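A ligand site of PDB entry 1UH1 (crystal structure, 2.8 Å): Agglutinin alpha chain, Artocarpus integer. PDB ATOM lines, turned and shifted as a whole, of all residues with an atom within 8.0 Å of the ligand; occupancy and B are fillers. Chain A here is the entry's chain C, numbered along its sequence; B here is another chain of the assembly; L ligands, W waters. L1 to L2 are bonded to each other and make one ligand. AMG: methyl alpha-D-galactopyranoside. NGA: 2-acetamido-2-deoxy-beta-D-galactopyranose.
OH of Tyr 78 sits close to O1 of AMG L1, at 3.4 Å. The backbone NH (N) of Tyr 122 is in hydrogen-bond range of an oxygen (O5) of AMG L1 (3.1 Å). The backbone NH (N) of Gly 1 sits at hydrogen-bond distance from an oxygen (O7) of NGA L2, at 2.7 Å. N of Trp 123 is in hydrogen-bond range of O6 of AMG L1 (3.0 Å). An oxygen (O4) of AMG L1 is in hydrogen-bond range of the side-chain carboxylate (OD1) of Asp 125, 2.7 Å away. The backbone carbonyl oxygen of Trp 123 sits at hydrogen-bond distance from an oxygen (O6) of AMG L1 (3.2 Å).
O of Asp 125 is in hydrogen-bond range of N of Ala 17 of chain B, at 2.8 Å. The backbone NH (N) of Gly 1 sits close to the side-chain carboxylate (OD2) of Asp 125. N of Gly 121 lies within hydrogen-bond range of OD2 of Asp 125 (3.4 Å). O of Gly 121 is in hydrogen-bond range of N of Phe 47 (2.8 Å). The backbone NH (N) of Asp 125 is in hydrogen-bond range of the backbone carbonyl oxygen (O) of Ser 119 (2.8 Å). The side-chain hydroxyl (OG) of Ser 119 sits close to the backbone carbonyl oxygen (O) of Gly 1, 3.5 Å away. The side-chain hydroxyl of Ser 46 is in hydrogen-bond range of the backbone carbonyl oxygen of Tyr 122 (2.7 Å).
CG1 of Val 80 touches C6 of AMG L1, at 3.9 Å. Gly 121 touches the ligand. Hydrophobic or aromatic side chains that line the ligand: Tyr 78, Val 80, Tyr 122 and Trp 123. Seven residues have an atom within 4 Å of the ligand: Gly 1, Tyr 78, Val 80, Gly 121, Tyr 122, Trp 123 and Asp 125. The nearest printed residue that does not touch the ligand is Phe 47 (4.3 Å).
Water W1 lies within hydrogen-bond range of N of Val 79 (3.0 Å) and O6 of NGA L2 (3.1 Å).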
ATOM      1  N   GLY A   1      24.094  16.334 -10.998  1.00  0.00           N
ATOM      2  CA  GLY A   1      23.013  15.304 -11.212  1.00  0.00           C
ATOM      3  C   GLY A   1      22.675  14.640  -9.880  1.00  0.00           C
ATOM      4  O   GLY A   1      23.221  14.998  -8.877  1.00  0.00           O
ATOM      5  N   LYS A   2      21.744  13.699  -9.865  1.00  0.00           N
ATOM      6  CA  LYS A   2      21.408  13.053  -8.626  1.00  0.00           C
ATOM      7  C   LYS A   2      22.264  11.817  -8.442  1.00  0.00           C
ATOM      8  O   LYS A   2      22.263  10.946  -9.306  1.00  0.00           O
ATOM      9  CB  LYS A   2      19.953  12.667  -8.656  1.00  0.00           C
ATOM     10  CG  LYS A   2      19.653  11.628  -7.663  1.00  0.00           C
ATOM     11  CD  LYS A   2      18.242  11.651  -7.349  1.00  0.00           C
ATOM     12  CE  LYS A   2      18.011  11.177  -5.960  1.00  0.00           C
ATOM     13  NZ  LYS A   2      16.646  10.542  -5.706  1.00  0.00           N
ATOM     14  N   ALA A   3      22.926  11.734  -7.295  1.00  0.00           N
ATOM     15  CA  ALA A   3      23.785  10.632  -6.979  1.00  0.00           C
ATOM     16  C   ALA A   3      23.048   9.371  -6.578  1.00  0.00           C
ATOM     17  O   ALA A   3      21.927   9.403  -6.067  1.00  0.00           O
ATOM     18  CB  ALA A   3      24.716  11.037  -5.881  1.00  0.00           C
ATOM     19  N   ALA A  24      25.733  11.441 -24.715  1.00  0.00           N
ATOM     20  CA  ALA A  24      26.421  10.516 -23.817  1.00  0.00           C
ATOM     21  C   ALA A  24      25.495   9.441 -23.258  1.00  0.00           C
ATOM     22  O   ALA A  24      24.436   9.155 -23.834  1.00  0.00           O
ATOM     23  CB  ALA A  24      27.067  11.278 -22.677  1.00  0.00           C
ATOM     24  N   ILE A  25      25.893   8.844 -22.136  1.00  0.00           N
ATOM     25  CA  ILE A  25      25.091   7.794 -21.499  1.00  0.00           C
ATOM     26  C   ILE A  25      23.933   8.413 -20.709  1.00  0.00           C
ATOM     27  O   ILE A  25      24.106   9.413 -20.027  1.00  0.00           O
ATOM     28  CB  ILE A  25      25.939   6.945 -20.550  1.00  0.00           C
ATOM     29  CG1 ILE A  25      27.070   6.259 -21.329  1.00  0.00           C
ATOM     30  CG2 ILE A  25      25.058   5.906 -19.850  1.00  0.00           C
ATOM     31  CD1 ILE A  25      26.589   5.279 -22.371  1.00  0.00           C
ATOM     32  N   SER A  46      17.853   9.580 -16.285  1.00  0.00           N
ATOM     33  CA  SER A  46      18.293  10.899 -16.705  1.00  0.00           C
ATOM     34  C   SER A  46      17.180  11.904 -16.484  1.00  0.00           C
ATOM     35  O   SER A  46      16.006  11.553 -16.479  1.00  0.00           O
ATOM     36  CB  SER A  46      18.655  10.863 -18.190  1.00  0.00           C
ATOM     37  OG  SER A  46      18.645  12.174 -18.736  1.00  0.00           O
ATOM     38  N   PHE A  47      17.554  13.168 -16.310  1.00  0.00           N
ATOM     39  CA  PHE A  47      16.578  14.226 -16.106  1.00  0.00           C
ATOM     40  C   PHE A  47      15.780  14.448 -17.383  1.00  0.00           C
ATOM     41  O   PHE A  47      14.680  15.000 -17.345  1.00  0.00           O
ATOM     42  CB  PHE A  47      17.260  15.526 -15.712  1.00  0.00           C
ATOM     43  CG  PHE A  47      17.918  15.491 -14.347  1.00  0.00           C
ATOM     44  CD1 PHE A  47      17.670  14.452 -13.456  1.00  0.00           C
ATOM     45  CD2 PHE A  47      18.743  16.534 -13.938  1.00  0.00           C
ATOM     46  CE1 PHE A  47      18.231  14.460 -12.180  1.00  0.00           C
ATOM     47  CE2 PHE A  47      19.306  16.547 -12.676  1.00  0.00           C
ATOM     48  CZ  PHE A  47      19.050  15.515 -11.799  1.00  0.00           C
ATOM     49  N   ILE A  48      16.343  14.009 -18.504  1.00  0.00           N
ATOM     50  CA  ILE A  48      15.695  14.150 -19.811  1.00  0.00           C
ATOM     51  C   ILE A  48      15.434  12.785 -20.462  1.00  0.00           C
ATOM     52  O   ILE A  48      15.784  11.750 -19.910  1.00  0.00           O
ATOM     53  CB  ILE A  48      16.553  14.993 -20.762  1.00  0.00           C
ATOM     54  CG1 ILE A  48      17.884  14.288 -21.032  1.00  0.00           C
ATOM     55  CG2 ILE A  48      16.791  16.376 -20.153  1.00  0.00           C
ATOM     56  CD1 ILE A  48      18.828  15.081 -21.891  1.00  0.00           C
ATOM     57  N   VAL A  75      30.127  17.758 -22.620  1.00  0.00           N
ATOM     58  CA  VAL A  75      28.834  17.894 -23.282  1.00  0.00           C
ATOM     59  C   VAL A  75      28.091  19.051 -22.620  1.00  0.00           C
ATOM     60  O   VAL A  75      27.760  18.994 -21.440  1.00  0.00           O
ATOM     61  CB  VAL A  75      27.987  16.598 -23.157  1.00  0.00           C
ATOM     62  CG1 VAL A  75      26.613  16.811 -23.780  1.00  0.00           C
ATOM     63  CG2 VAL A  75      28.702  15.449 -23.835  1.00  0.00           C
ATOM     64  N   SER A  76      27.840  20.115 -23.387  1.00  0.00           N
ATOM     65  CA  SER A  76      27.180  21.313 -22.883  1.00  0.00           C
ATOM     66  C   SER A  76      27.926  21.848 -21.691  1.00  0.00           C
ATOM     67  O   SER A  76      27.328  22.353 -20.749  1.00  0.00           O
ATOM     68  CB  SER A  76      25.729  21.031 -22.480  1.00  0.00           C
ATOM     69  OG  SER A  76      24.905  20.950 -23.625  1.00  0.00           O
ATOM     70  N   GLY A  77      29.243  21.703 -21.721  1.00  0.00           N
ATOM     71  CA  GLY A  77      30.051  22.215 -20.632  1.00  0.00           C
ATOM     72  C   GLY A  77      30.166  21.335 -19.401  1.00  0.00           C
ATOM     73  O   GLY A  77      30.832  21.725 -18.452  1.00  0.00           O
ATOM     74  N   TYR A  78      29.515  20.174 -19.404  1.00  0.00           N
ATOM     75  CA  TYR A  78      29.589  19.267 -18.263  1.00  0.00           C
ATOM     76  C   TYR A  78      30.445  18.075 -18.632  1.00  0.00           C
ATOM     77  O   TYR A  78      30.343  17.537 -19.727  1.00  0.00           O
ATOM     78  CB  TYR A  78      28.205  18.748 -17.872  1.00  0.00           C
ATOM     79  CG  TYR A  78      27.240  19.819 -17.425  1.00  0.00           C
ATOM     80  CD1 TYR A  78      27.253  20.303 -16.125  1.00  0.00           C
ATOM     81  CD2 TYR A  78      26.303  20.333 -18.321  1.00  0.00           C
ATOM     82  CE1 TYR A  78      26.359  21.298 -15.717  1.00  0.00           C
ATOM     83  CE2 TYR A  78      25.401  21.336 -17.928  1.00  0.00           C
ATOM     84  CZ  TYR A  78      25.433  21.808 -16.622  1.00  0.00           C
ATOM     85  OH  TYR A  78      24.551  22.796 -16.233  1.00  0.00           O
ATOM     86  N   VAL A  79      31.305  17.649 -17.722  1.00  0.00           N
ATOM     87  CA  VAL A  79      32.129  16.478 -17.985  1.00  0.00           C
ATOM     88  C   VAL A  79      31.279  15.259 -17.622  1.00  0.00           C
ATOM     89  O   VAL A  79      30.801  15.140 -16.508  1.00  0.00           O
ATOM     90  CB  VAL A  79      33.397  16.469 -17.127  1.00  0.00           C
ATOM     91  CG1 VAL A  79      34.147  15.185 -17.343  1.00  0.00           C
ATOM     92  CG2 VAL A  79      34.256  17.627 -17.509  1.00  0.00           C
ATOM     93  N   VAL A  80      31.086  14.363 -18.581  1.00  0.00           N
ATOM     94  CA  VAL A  80      30.262  13.184 -18.337  1.00  0.00           C
ATOM     95  C   VAL A  80      30.858  11.951 -18.985  1.00  0.00           C
ATOM     96  O   VAL A  80      31.850  12.028 -19.710  1.00  0.00           O
ATOM     97  CB  VAL A  80      28.840  13.379 -18.904  1.00  0.00           C
ATOM     98  CG1 VAL A  80      28.127  14.505 -18.174  1.00  0.00           C
ATOM     99  CG2 VAL A  80      28.912  13.658 -20.407  1.00  0.00           C
ATOM    100  N   VAL A  81      30.235  10.813 -18.715  1.00  0.00           N
ATOM    101  CA  VAL A  81      30.670   9.555 -19.305  1.00  0.00           C
ATOM    102  C   VAL A  81      29.940   9.472 -20.633  1.00  0.00           C
ATOM    103  O   VAL A  81      28.726   9.218 -20.668  1.00  0.00           O
ATOM    104  CB  VAL A  81      30.279   8.368 -18.394  1.00  0.00           C
ATOM    105  CG1 VAL A  81      30.735   7.063 -19.017  1.00  0.00           C
ATOM    106  CG2 VAL A  81      30.901   8.551 -17.028  1.00  0.00           C
ATOM    107  N   SER A 119      26.461   9.160 -10.475  1.00  0.00           N
ATOM    108  CA  SER A 119      25.569  10.308 -10.500  1.00  0.00           C
ATOM    109  C   SER A 119      24.995  10.507 -11.886  1.00  0.00           C
ATOM    110  O   SER A 119      25.668  10.271 -12.890  1.00  0.00           O
ATOM    111  CB  SER A 119      26.313  11.553 -10.058  1.00  0.00           C
ATOM    112  OG  SER A 119      25.482  12.695 -10.171  1.00  0.00           O
ATOM    113  N   ILE A 120      23.739  10.943 -11.949  1.00  0.00           N
ATOM    114  CA  ILE A 120      23.092  11.157 -13.230  1.00  0.00           C
ATOM    115  C   ILE A 120      22.235  12.405 -13.235  1.00  0.00           C
ATOM    116  O   ILE A 120      21.336  12.573 -12.400  1.00  0.00           O
ATOM    117  CB  ILE A 120      22.204   9.945 -13.623  1.00  0.00           C
ATOM    118  CG1 ILE A 120      23.055   8.685 -13.742  1.00  0.00           C
ATOM    119  CG2 ILE A 120      21.484  10.220 -14.935  1.00  0.00           C
ATOM    120  CD1 ILE A 120      22.251   7.441 -14.020  1.00  0.00           C
ATOM    121  N   GLY A 121      22.528  13.297 -14.163  1.00  0.00           N
ATOM    122  CA  GLY A 121      21.749  14.509 -14.331  1.00  0.00           C
ATOM    123  C   GLY A 121      21.135  14.294 -15.694  1.00  0.00           C
ATOM    124  O   GLY A 121      20.282  13.428 -15.860  1.00  0.00           O
ATOM    125  N   TYR A 122      21.558  15.068 -16.672  1.00  0.00           N
ATOM    126  CA  TYR A 122      21.056  14.876 -18.023  1.00  0.00           C
ATOM    127  C   TYR A 122      21.761  13.625 -18.513  1.00  0.00           C
ATOM    128  O   TYR A 122      21.211  12.845 -19.294  1.00  0.00           O
ATOM    129  CB  TYR A 122      21.456  16.066 -18.924  1.00  0.00           C
ATOM    130  CG  TYR A 122      20.515  17.239 -18.866  1.00  0.00           C
ATOM    131  CD1 TYR A 122      19.899  17.610 -17.683  1.00  0.00           C
ATOM    132  CD2 TYR A 122      20.260  17.985 -20.008  1.00  0.00           C
ATOM    133  CE1 TYR A 122      19.054  18.710 -17.621  1.00  0.00           C
ATOM    134  CE2 TYR A 122      19.418  19.087 -19.969  1.00  0.00           C
ATOM    135  CZ  TYR A 122      18.810  19.439 -18.777  1.00  0.00           C
ATOM    136  OH  TYR A 122      17.966  20.522 -18.730  1.00  0.00           O
ATOM    137  N   TRP A 123      22.985  13.447 -18.047  1.00  0.00           N
ATOM    138  CA  TRP A 123      23.796  12.308 -18.430  1.00  0.00           C
ATOM    139  C   TRP A 123      24.509  11.739 -17.224  1.00  0.00           C
ATOM    140  O   TRP A 123      24.462  12.303 -16.131  1.00  0.00           O
ATOM    141  CB  TRP A 123      24.821  12.744 -19.480  1.00  0.00           C
ATOM    142  CG  TRP A 123      24.170  13.380 -20.662  1.00  0.00           C
ATOM    143  CD1 TRP A 123      23.400  12.774 -21.615  1.00  0.00           C
ATOM    144  CD2 TRP A 123      24.149  14.786 -20.978  1.00  0.00           C
ATOM    145  NE1 TRP A 123      22.891  13.697 -22.495  1.00  0.00           N
ATOM    146  CE2 TRP A 123      23.339  14.943 -22.114  1.00  0.00           C
ATOM    147  CE3 TRP A 123      24.725  15.912 -20.389  1.00  0.00           C
ATOM    148  CZ2 TRP A 123      23.100  16.198 -22.705  1.00  0.00           C
ATOM    149  CZ3 TRP A 123      24.484  17.161 -20.967  1.00  0.00           C
ATOM    150  CH2 TRP A 123      23.673  17.282 -22.112  1.00  0.00           C
ATOM    151  N   LEU A 124      25.147  10.599 -17.430  1.00  0.00           N
ATOM    152  CA  LEU A 124      25.882   9.945 -16.361  1.00  0.00           C
ATOM    153  C   LEU A 124      27.096  10.808 -16.094  1.00  0.00           C
ATOM    154  O   LEU A 124      28.026  10.864 -16.892  1.00  0.00           O
ATOM    155  CB  LEU A 124      26.302   8.542 -16.823  1.00  0.00           C
ATOM    156  CG  LEU A 124      27.174   7.674 -15.918  1.00  0.00           C
ATOM    157  CD1 LEU A 124      26.487   7.405 -14.576  1.00  0.00           C
ATOM    158  CD2 LEU A 124      27.441   6.373 -16.648  1.00  0.00           C
ATOM    159  N   ASP A 125      27.084  11.510 -14.964  1.00  0.00           N
ATOM    160  CA  ASP A 125      28.186  12.390 -14.596  1.00  0.00           C
ATOM    161  C   ASP A 125      29.488  11.652 -14.320  1.00  0.00           C
ATOM    162  O   ASP A 125      30.561  12.047 -14.792  1.00  0.00           O
ATOM    163  CB  ASP A 125      27.797  13.222 -13.370  1.00  0.00           C
ATOM    164  CG  ASP A 125      26.520  13.991 -13.581  1.00  0.00           C
ATOM    165  OD1 ASP A 125      26.459  14.776 -14.557  1.00  0.00           O
ATOM    166  OD2 ASP A 125      25.564  13.829 -12.788  1.00  0.00           O
ATOM    167  N   TYR A 126      29.393  10.577 -13.539  1.00  0.00           N
ATOM    168  CA  TYR A 126      30.548   9.779 -13.180  1.00  0.00           C
ATOM    169  C   TYR A 126      30.054   8.515 -12.539  1.00  0.00           C
ATOM    170  O   TYR A 126      28.857   8.397 -12.227  1.00  0.00           O
ATOM    171  CB  TYR A 126      31.426  10.546 -12.191  1.00  0.00           C
ATOM    172  CG  TYR A 126      30.725  10.900 -10.902  1.00  0.00           C
ATOM    173  CD1 TYR A 126      30.461   9.929  -9.919  1.00  0.00           C
ATOM    174  CD2 TYR A 126      30.296  12.202 -10.660  1.00  0.00           C
ATOM    175  CE1 TYR A 126      29.783  10.259  -8.748  1.00  0.00           C
ATOM    176  CE2 TYR A 126      29.620  12.538  -9.501  1.00  0.00           C
ATOM    177  CZ  TYR A 126      29.370  11.574  -8.553  1.00  0.00           C
ATOM    178  OH  TYR A 126      28.686  11.917  -7.408  1.00  0.00           O
ATOM    179  N   ALA B  17      32.956  13.376 -14.357  1.00  0.00           N
ATOM    180  CA  ALA B  17      33.008  14.676 -13.682  1.00  0.00           C
ATOM    181  C   ALA B  17      33.801  14.608 -12.366  1.00  0.00           C
ATOM    182  O   ALA B  17      33.635  13.681 -11.584  1.00  0.00           O
ATOM    183  CB  ALA B  17      31.604  15.176 -13.407  1.00  0.00           C
ATOM    184  N   LYS B  18      34.646  15.603 -12.142  1.00  0.00           N
ATOM    185  CA  LYS B  18      35.460  15.655 -10.933  1.00  0.00           C
ATOM    186  C   LYS B  18      34.576  15.881  -9.700  1.00  0.00           C
ATOM    187  O   LYS B  18      34.591  15.021  -8.796  1.00  0.00           O
ATOM    188  CB  LYS B  18      36.487  16.783 -11.052  1.00  0.00           C
ATOM    189  CG  LYS B  18      37.621  16.741 -10.034  1.00  0.00           C
ATOM    190  CD  LYS B  18      38.688  15.703 -10.387  1.00  0.00           C
ATOM    191  CE  LYS B  18      38.175  14.264 -10.262  1.00  0.00           C
ATOM    192  NZ  LYS B  18      37.751  13.940  -8.873  1.00  0.00           N
HETATM  193  C1  AMG L   1      22.443  18.778 -15.414  1.00  0.00           C
HETATM  194  C2  AMG L   1      22.716  18.838 -13.994  1.00  0.00           C
HETATM  195  C3  AMG L   1      24.295  18.990 -13.778  1.00  0.00           C
HETATM  196  C4  AMG L   1      25.046  17.814 -14.517  1.00  0.00           C
HETATM  197  C5  AMG L   1      24.617  17.754 -15.985  1.00  0.00           C
HETATM  198  C6  AMG L   1      25.216  16.700 -16.904  1.00  0.00           C
HETATM  199  C7  AMG L   1      22.221  20.108 -17.587  1.00  0.00           C
HETATM  200  O1  AMG L   1      22.708  19.971 -16.201  1.00  0.00           O
HETATM  201  O2  AMG L   1      22.097  19.889 -13.323  1.00  0.00           O
HETATM  202  O3  AMG L   1      24.473  18.918 -12.307  1.00  0.00           O
HETATM  203  O4  AMG L   1      24.640  16.667 -13.794  1.00  0.00           O
HETATM  204  O5  AMG L   1      23.151  17.682 -16.006  1.00  0.00           O
HETATM  205  O6  AMG L   1      24.686  15.434 -16.545  1.00  0.00           O
HETATM  206  C1  NGA L   2      25.118  19.774 -11.760  1.00  0.00           C
HETATM  207  C2  NGA L   2      24.899  19.915 -10.236  1.00  0.00           C
HETATM  208  C3  NGA L   2      25.957  20.908  -9.689  1.00  0.00           C
HETATM  209  C4  NGA L   2      27.434  20.333  -9.940  1.00  0.00           C
HETATM  210  C5  NGA L   2      27.658  20.295 -11.534  1.00  0.00           C
HETATM  211  C6  NGA L   2      29.046  19.773 -11.931  1.00  0.00           C
HETATM  212  C7  NGA L   2      22.392  19.556 -10.069  1.00  0.00           C
HETATM  213  C8  NGA L   2      21.062  20.248  -9.891  1.00  0.00           C
HETATM  214  N2  NGA L   2      23.546  20.368 -10.078  1.00  0.00           N
HETATM  215  O3  NGA L   2      25.744  21.003  -8.319  1.00  0.00           O
HETATM  216  O4  NGA L   2      27.571  19.034  -9.353  1.00  0.00           O
HETATM  217  O5  NGA L   2      26.522  19.359 -12.066  1.00  0.00           O
HETATM  218  O6  NGA L   2      29.184  19.530 -13.349  1.00  0.00           O
HETATM  219  O7  NGA L   2      22.402  18.320 -10.226  1.00  0.00           O
HETATM  220  O   HOH W   1      31.680  18.769 -15.006  1.00  0.00           O
